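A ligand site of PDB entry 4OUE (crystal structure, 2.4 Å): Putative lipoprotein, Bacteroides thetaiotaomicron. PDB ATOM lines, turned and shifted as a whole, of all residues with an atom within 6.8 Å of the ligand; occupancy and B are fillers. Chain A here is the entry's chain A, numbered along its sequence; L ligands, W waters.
The side-chain carboxylate (OE1) of Glu 232 lies within hydrogen-bond range of an oxygen (O1) of the ligand. O5 of the ligand is in hydrogen-bond range of OD2 of Asp 255 (2.6 Å). The side-chain carboxylate of Glu 212 lies within hydrogen-bond range of an oxygen (O5) of the ligand (2.7 Å). OD1 of Asp 166 is in hydrogen-bond range of O3 of the ligand, 2.9 Å away. An oxygen (O3) of the ligand sits at hydrogen-bond distance from the backbone NH (N) of Gly 167 (3.0 Å). NE1 of Trp 208 is in hydrogen-bond range of O5 of the ligand (3.4 Å).
The side-chain carboxylate (OD1) of Asp 255 sits at hydrogen-bond distance from the indole nitrogen (NE1) of Trp 208 (3.0 Å). The indole nitrogen (NE1) of Trp 262 is in hydrogen-bond range of the side-chain carboxylate (OE1) of Glu 212, 3.3 Å away. The side-chain carboxylate (OD1) of Asp 166 lies within hydrogen-bond range of the backbone NH (N) of Ala 168, at 3.0 Å. The backbone NH of Gly 167 lies within hydrogen-bond range of the side-chain hydroxyl of Thr 197. The side-chain amino group (NZ) of Lys 198 is in hydrogen-bond range of the backbone carbonyl oxygen (O) of Gly 167. The side-chain hydroxyl of Thr 197 is in hydrogen-bond range of the backbone carbonyl oxygen of Trp 165. The backbone carbonyl oxygen (O) of Asn 211 is in hydrogen-bond range of the indole nitrogen (NE1) of Trp 208 (3.1 Å). The backbone NH (N) of Lys 198 is in hydrogen-bond range of the backbone carbonyl oxygen (O) of Ile 229.
Residues that only touch the ligand: Trp 164 (3.8 Å), Ala 168 (3.7 Å), Thr 197 (3.3 Å) and Lys 198 (3.7 Å). Hydrophobic or aromatic side chains within 4 Å of the ligand: Trp 164, Ala 168 and Trp 208. Within 4 Å of the ligand: Trp 164, Asp 166, Gly 167, Ala 168, Thr 197, Lys 198, Trp 208, Glu 212, Glu 232 and Asp 255.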
ATOM      1  N   PHE A  25       4.035 -10.118 -21.670  1.00  0.00           N
ATOM      2  CA  PHE A  25       4.946 -10.339 -22.786  1.00  0.00           C
ATOM      3  C   PHE A  25       4.438  -9.434 -23.913  1.00  0.00           C
ATOM      4  O   PHE A  25       3.215  -9.276 -24.084  1.00  0.00           O
ATOM      5  CB  PHE A  25       4.846 -11.798 -23.220  1.00  0.00           C
ATOM      6  CG  PHE A  25       6.176 -12.513 -23.381  1.00  0.00           C
ATOM      7  CD1 PHE A  25       7.352 -11.831 -23.639  1.00  0.00           C
ATOM      8  CD2 PHE A  25       6.212 -13.910 -23.304  1.00  0.00           C
ATOM      9  CE1 PHE A  25       8.564 -12.520 -23.804  1.00  0.00           C
ATOM     10  CE2 PHE A  25       7.412 -14.606 -23.468  1.00  0.00           C
ATOM     11  CZ  PHE A  25       8.588 -13.910 -23.706  1.00  0.00           C
ATOM     12  N   TYR A 123      13.489  -9.509 -23.883  1.00  0.00           N
ATOM     13  CA  TYR A 123      13.681 -10.795 -24.553  1.00  0.00           C
ATOM     14  C   TYR A 123      14.668 -10.548 -25.701  1.00  0.00           C
ATOM     15  O   TYR A 123      14.405  -9.737 -26.583  1.00  0.00           O
ATOM     16  CB  TYR A 123      12.335 -11.316 -25.079  1.00  0.00           C
ATOM     17  CG  TYR A 123      12.328 -12.541 -25.980  1.00  0.00           C
ATOM     18  CD1 TYR A 123      11.638 -13.688 -25.601  1.00  0.00           C
ATOM     19  CD2 TYR A 123      12.934 -12.539 -27.234  1.00  0.00           C
ATOM     20  CE1 TYR A 123      11.579 -14.806 -26.424  1.00  0.00           C
ATOM     21  CE2 TYR A 123      12.896 -13.650 -28.061  1.00  0.00           C
ATOM     22  CZ  TYR A 123      12.214 -14.783 -27.642  1.00  0.00           C
ATOM     23  OH  TYR A 123      12.164 -15.889 -28.473  1.00  0.00           O
ATOM     24  N   TRP A 164      15.246 -12.556 -20.889  1.00  0.00           N
ATOM     25  CA  TRP A 164      14.590 -13.794 -21.279  1.00  0.00           C
ATOM     26  C   TRP A 164      15.386 -14.528 -22.362  1.00  0.00           C
ATOM     27  O   TRP A 164      15.643 -13.973 -23.439  1.00  0.00           O
ATOM     28  CB  TRP A 164      13.199 -13.491 -21.814  1.00  0.00           C
ATOM     29  CG  TRP A 164      12.111 -14.414 -21.302  1.00  0.00           C
ATOM     30  CD1 TRP A 164      11.474 -14.343 -20.091  1.00  0.00           C
ATOM     31  CD2 TRP A 164      11.513 -15.505 -22.014  1.00  0.00           C
ATOM     32  NE1 TRP A 164      10.526 -15.351 -19.999  1.00  0.00           N
ATOM     33  CE2 TRP A 164      10.533 -16.063 -21.171  1.00  0.00           C
ATOM     34  CE3 TRP A 164      11.716 -16.052 -23.285  1.00  0.00           C
ATOM     35  CZ2 TRP A 164       9.744 -17.147 -21.560  1.00  0.00           C
ATOM     36  CZ3 TRP A 164      10.942 -17.133 -23.665  1.00  0.00           C
ATOM     37  CH2 TRP A 164       9.962 -17.676 -22.803  1.00  0.00           C
ATOM     38  N   TRP A 165      15.767 -15.768 -22.057  1.00  0.00           N
ATOM     39  CA  TRP A 165      16.533 -16.572 -23.012  1.00  0.00           C
ATOM     40  C   TRP A 165      15.697 -17.753 -23.533  1.00  0.00           C
ATOM     41  O   TRP A 165      15.600 -18.815 -22.888  1.00  0.00           O
ATOM     42  CB  TRP A 165      17.842 -17.061 -22.384  1.00  0.00           C
ATOM     43  CG  TRP A 165      18.881 -15.985 -22.255  1.00  0.00           C
ATOM     44  CD1 TRP A 165      18.940 -14.799 -22.950  1.00  0.00           C
ATOM     45  CD2 TRP A 165      20.023 -15.995 -21.387  1.00  0.00           C
ATOM     46  NE1 TRP A 165      20.046 -14.088 -22.556  1.00  0.00           N
ATOM     47  CE2 TRP A 165      20.733 -14.788 -21.608  1.00  0.00           C
ATOM     48  CE3 TRP A 165      20.523 -16.912 -20.456  1.00  0.00           C
ATOM     49  CZ2 TRP A 165      21.916 -14.482 -20.915  1.00  0.00           C
ATOM     50  CZ3 TRP A 165      21.703 -16.602 -19.772  1.00  0.00           C
ATOM     51  CH2 TRP A 165      22.380 -15.396 -19.993  1.00  0.00           C
ATOM     52  N   ASP A 166      15.105 -17.565 -24.702  1.00  0.00           N
ATOM     53  CA  ASP A 166      14.348 -18.606 -25.366  1.00  0.00           C
ATOM     54  C   ASP A 166      15.306 -19.736 -25.743  1.00  0.00           C
ATOM     55  O   ASP A 166      16.404 -19.479 -26.244  1.00  0.00           O
ATOM     56  CB  ASP A 166      13.669 -18.024 -26.621  1.00  0.00           C
ATOM     57  CG  ASP A 166      12.474 -18.844 -27.091  1.00  0.00           C
ATOM     58  OD1 ASP A 166      12.504 -20.101 -27.017  1.00  0.00           O
ATOM     59  OD2 ASP A 166      11.472 -18.231 -27.545  1.00  0.00           O
ATOM     60  N   GLY A 167      14.895 -20.975 -25.479  1.00  0.00           N
ATOM     61  CA  GLY A 167      15.732 -22.124 -25.776  1.00  0.00           C
ATOM     62  C   GLY A 167      15.459 -22.716 -27.154  1.00  0.00           C
ATOM     63  O   GLY A 167      16.139 -23.662 -27.571  1.00  0.00           O
ATOM     64  N   ALA A 168      14.484 -22.158 -27.863  1.00  0.00           N
ATOM     65  CA  ALA A 168      14.171 -22.623 -29.216  1.00  0.00           C
ATOM     66  C   ALA A 168      15.339 -22.382 -30.168  1.00  0.00           C
ATOM     67  O   ALA A 168      15.761 -21.237 -30.381  1.00  0.00           O
ATOM     68  CB  ALA A 168      12.930 -21.927 -29.743  1.00  0.00           C
ATOM     69  N   GLY A 169      15.862 -23.463 -30.735  1.00  0.00           N
ATOM     70  CA  GLY A 169      16.950 -23.385 -31.701  1.00  0.00           C
ATOM     71  C   GLY A 169      18.318 -23.080 -31.111  1.00  0.00           C
ATOM     72  O   GLY A 169      19.274 -22.865 -31.858  1.00  0.00           O
ATOM     73  N   PHE A 195      15.552 -15.639 -17.077  1.00  0.00           N
ATOM     74  CA  PHE A 195      14.802 -16.822 -17.475  1.00  0.00           C
ATOM     75  C   PHE A 195      15.746 -17.656 -18.306  1.00  0.00           C
ATOM     76  O   PHE A 195      16.008 -17.329 -19.463  1.00  0.00           O
ATOM     77  CB  PHE A 195      13.580 -16.429 -18.307  1.00  0.00           C
ATOM     78  CG  PHE A 195      12.808 -17.605 -18.860  1.00  0.00           C
ATOM     79  CD1 PHE A 195      11.845 -18.251 -18.084  1.00  0.00           C
ATOM     80  CD2 PHE A 195      13.025 -18.055 -20.154  1.00  0.00           C
ATOM     81  CE1 PHE A 195      11.124 -19.324 -18.599  1.00  0.00           C
ATOM     82  CE2 PHE A 195      12.302 -19.123 -20.677  1.00  0.00           C
ATOM     83  CZ  PHE A 195      11.352 -19.753 -19.897  1.00  0.00           C
ATOM     84  N   GLY A 196      16.283 -18.708 -17.690  1.00  0.00           N
ATOM     85  CA  GLY A 196      17.279 -19.543 -18.349  1.00  0.00           C
ATOM     86  C   GLY A 196      16.776 -20.887 -18.863  1.00  0.00           C
ATOM     87  O   GLY A 196      16.048 -21.612 -18.179  1.00  0.00           O
ATOM     88  N   THR A 197      17.206 -21.237 -20.070  1.00  0.00           N
ATOM     89  CA  THR A 197      16.851 -22.523 -20.665  1.00  0.00           C
ATOM     90  C   THR A 197      18.089 -23.290 -21.134  1.00  0.00           C
ATOM     91  O   THR A 197      19.144 -22.695 -21.420  1.00  0.00           O
ATOM     92  CB  THR A 197      15.901 -22.341 -21.854  1.00  0.00           C
ATOM     93  OG1 THR A 197      16.461 -21.369 -22.749  1.00  0.00           O
ATOM     94  CG2 THR A 197      14.529 -21.861 -21.388  1.00  0.00           C
ATOM     95  N   LYS A 198      17.966 -24.610 -21.196  1.00  0.00           N
ATOM     96  CA  LYS A 198      19.029 -25.472 -21.714  1.00  0.00           C
ATOM     97  C   LYS A 198      20.438 -25.177 -21.156  1.00  0.00           C
ATOM     98  O   LYS A 198      20.649 -25.245 -19.940  1.00  0.00           O
ATOM     99  CB  LYS A 198      18.998 -25.459 -23.239  1.00  0.00           C
ATOM    100  CG  LYS A 198      17.666 -25.991 -23.752  1.00  0.00           C
ATOM    101  CD  LYS A 198      17.514 -25.856 -25.262  1.00  0.00           C
ATOM    102  CE  LYS A 198      16.201 -26.483 -25.703  1.00  0.00           C
ATOM    103  NZ  LYS A 198      15.956 -26.323 -27.155  1.00  0.00           N
ATOM    104  N   TRP A 208      11.706 -22.660 -17.368  1.00  0.00           N
ATOM    105  CA  TRP A 208      10.491 -22.954 -18.115  1.00  0.00           C
ATOM    106  C   TRP A 208       9.776 -24.103 -17.430  1.00  0.00           C
ATOM    107  O   TRP A 208      10.378 -24.866 -16.665  1.00  0.00           O
ATOM    108  CB  TRP A 208      10.853 -23.343 -19.547  1.00  0.00           C
ATOM    109  CG  TRP A 208       9.643 -23.475 -20.433  1.00  0.00           C
ATOM    110  CD1 TRP A 208       8.516 -22.683 -20.433  1.00  0.00           C
ATOM    111  CD2 TRP A 208       9.433 -24.464 -21.442  1.00  0.00           C
ATOM    112  NE1 TRP A 208       7.637 -23.120 -21.402  1.00  0.00           N
ATOM    113  CE2 TRP A 208       8.177 -24.214 -22.030  1.00  0.00           C
ATOM    114  CE3 TRP A 208      10.202 -25.535 -21.923  1.00  0.00           C
ATOM    115  CZ2 TRP A 208       7.664 -24.995 -23.067  1.00  0.00           C
ATOM    116  CZ3 TRP A 208       9.686 -26.323 -22.940  1.00  0.00           C
ATOM    117  CH2 TRP A 208       8.429 -26.046 -23.512  1.00  0.00           C
ATOM    118  N   GLY A 210       7.757 -26.381 -19.271  1.00  0.00           N
ATOM    119  CA  GLY A 210       7.531 -27.500 -20.179  1.00  0.00           C
ATOM    120  C   GLY A 210       6.400 -27.392 -21.177  1.00  0.00           C
ATOM    121  O   GLY A 210       6.321 -28.205 -22.111  1.00  0.00           O
ATOM    122  N   ASN A 211       5.498 -26.427 -21.006  1.00  0.00           N
ATOM    123  CA  ASN A 211       4.471 -26.192 -22.029  1.00  0.00           C
ATOM    124  C   ASN A 211       4.128 -24.723 -22.234  1.00  0.00           C
ATOM    125  O   ASN A 211       4.583 -23.853 -21.486  1.00  0.00           O
ATOM    126  CB  ASN A 211       3.214 -27.021 -21.765  1.00  0.00           C
ATOM    127  CG  ASN A 211       2.458 -26.585 -20.526  1.00  0.00           C
ATOM    128  OD1 ASN A 211       1.702 -25.610 -20.557  1.00  0.00           O
ATOM    129  ND2 ASN A 211       2.649 -27.311 -19.427  1.00  0.00           N
ATOM    130  N   GLU A 212       3.332 -24.441 -23.266  1.00  0.00           N
ATOM    131  CA  GLU A 212       2.899 -23.082 -23.547  1.00  0.00           C
ATOM    132  C   GLU A 212       1.383 -22.966 -23.494  1.00  0.00           C
ATOM    133  O   GLU A 212       0.789 -22.162 -24.203  1.00  0.00           O
ATOM    134  CB  GLU A 212       3.414 -22.626 -24.914  1.00  0.00           C
ATOM    135  CG  GLU A 212       4.942 -22.515 -25.002  1.00  0.00           C
ATOM    136  CD  GLU A 212       5.426 -22.101 -26.381  1.00  0.00           C
ATOM    137  OE1 GLU A 212       4.628 -22.168 -27.342  1.00  0.00           O
ATOM    138  OE2 GLU A 212       6.610 -21.705 -26.512  1.00  0.00           O
ATOM    139  N   ILE A 229      16.690 -28.620 -16.674  1.00  0.00           N
ATOM    140  CA  ILE A 229      16.700 -27.424 -17.513  1.00  0.00           C
ATOM    141  C   ILE A 229      17.577 -27.658 -18.755  1.00  0.00           C
ATOM    142  O   ILE A 229      17.180 -27.355 -19.883  1.00  0.00           O
ATOM    143  CB  ILE A 229      17.227 -26.223 -16.691  1.00  0.00           C
ATOM    144  CG1 ILE A 229      16.244 -25.890 -15.572  1.00  0.00           C
ATOM    145  CG2 ILE A 229      17.474 -25.014 -17.595  1.00  0.00           C
ATOM    146  CD1 ILE A 229      16.783 -24.915 -14.556  1.00  0.00           C
ATOM    147  N   GLU A 232      16.262 -30.385 -21.383  1.00  0.00           N
ATOM    148  CA  GLU A 232      14.864 -29.982 -21.369  1.00  0.00           C
ATOM    149  C   GLU A 232      13.893 -30.992 -21.951  1.00  0.00           C
ATOM    150  O   GLU A 232      12.860 -31.297 -21.334  1.00  0.00           O
ATOM    151  CB  GLU A 232      14.758 -28.658 -22.132  1.00  0.00           C
ATOM    152  CG  GLU A 232      13.376 -28.109 -22.354  1.00  0.00           C
ATOM    153  CD  GLU A 232      13.438 -26.824 -23.174  1.00  0.00           C
ATOM    154  OE1 GLU A 232      12.962 -26.815 -24.328  1.00  0.00           O
ATOM    155  OE2 GLU A 232      13.970 -25.811 -22.650  1.00  0.00           O
ATOM    156  N   ASP A 255       4.483 -19.355 -19.280  1.00  0.00           N
ATOM    157  CA  ASP A 255       4.249 -18.431 -20.410  1.00  0.00           C
ATOM    158  C   ASP A 255       3.119 -18.883 -21.322  1.00  0.00           C
ATOM    159  O   ASP A 255       3.041 -20.050 -21.687  1.00  0.00           O
ATOM    160  CB  ASP A 255       5.523 -18.212 -21.233  1.00  0.00           C
ATOM    161  CG  ASP A 255       6.083 -19.506 -21.834  1.00  0.00           C
ATOM    162  OD1 ASP A 255       6.066 -20.562 -21.155  1.00  0.00           O
ATOM    163  OD2 ASP A 255       6.557 -19.468 -22.998  1.00  0.00           O
ATOM    164  N   TRP A 262       1.726 -16.179 -30.925  1.00  0.00           N
ATOM    165  CA  TRP A 262       2.495 -15.222 -30.133  1.00  0.00           C
ATOM    166  C   TRP A 262       2.499 -13.821 -30.761  1.00  0.00           C
ATOM    167  O   TRP A 262       2.455 -12.816 -30.047  1.00  0.00           O
ATOM    168  CB  TRP A 262       3.928 -15.731 -29.930  1.00  0.00           C
ATOM    169  CG  TRP A 262       4.034 -16.925 -28.999  1.00  0.00           C
ATOM    170  CD1 TRP A 262       4.257 -18.233 -29.358  1.00  0.00           C
ATOM    171  CD2 TRP A 262       3.967 -16.915 -27.559  1.00  0.00           C
ATOM    172  NE1 TRP A 262       4.328 -19.021 -28.239  1.00  0.00           N
ATOM    173  CE2 TRP A 262       4.155 -18.248 -27.117  1.00  0.00           C
ATOM    174  CE3 TRP A 262       3.788 -15.911 -26.595  1.00  0.00           C
ATOM    175  CZ2 TRP A 262       4.138 -18.601 -25.763  1.00  0.00           C
ATOM    176  CZ3 TRP A 262       3.789 -16.267 -25.249  1.00  0.00           C
ATOM    177  CH2 TRP A 262       3.960 -17.598 -24.848  1.00  0.00           C
HETATM  178  C1  LIG L   1      10.552 -23.893 -26.118  1.00  0.00           C
HETATM  179  C2  LIG L   1      11.996 -23.874 -25.784  1.00  0.00           C
HETATM  180  O1  LIG L   1      12.599 -25.054 -26.158  1.00  0.00           O
HETATM  181  C3  LIG L   1      12.137 -23.639 -24.305  1.00  0.00           C
HETATM  182  O2  LIG L   1      13.486 -23.564 -23.978  1.00  0.00           O
HETATM  183  C4  LIG L   1      11.410 -22.386 -23.906  1.00  0.00           C
HETATM  184  O3  LIG L   1      12.059 -21.279 -24.423  1.00  0.00           O
HETATM  185  C5  LIG L   1       9.998 -22.441 -24.438  1.00  0.00           C
HETATM  186  O4  LIG L   1      10.014 -22.646 -25.813  1.00  0.00           O
HETATM  187  C6  LIG L   1       9.299 -21.154 -24.138  1.00  0.00           C
HETATM  188  O5  LIG L   1       7.927 -21.323 -24.234  1.00  0.00           O
HETATM  189  S1  LIG L   1      10.362 -24.301 -27.842  1.00  0.00           S
HETATM  190  C7  LIG L   1       8.692 -24.816 -28.154  1.00  0.00           C
HETATM  191  C8  LIG L   1       8.599 -26.299 -28.281  1.00  0.00           C
HETATM  192  C9  LIG L   1       7.840 -24.465 -26.988  1.00  0.00           C
HETATM  193  O   HOH W   1       9.358 -20.991 -27.944  1.00  0.00           O
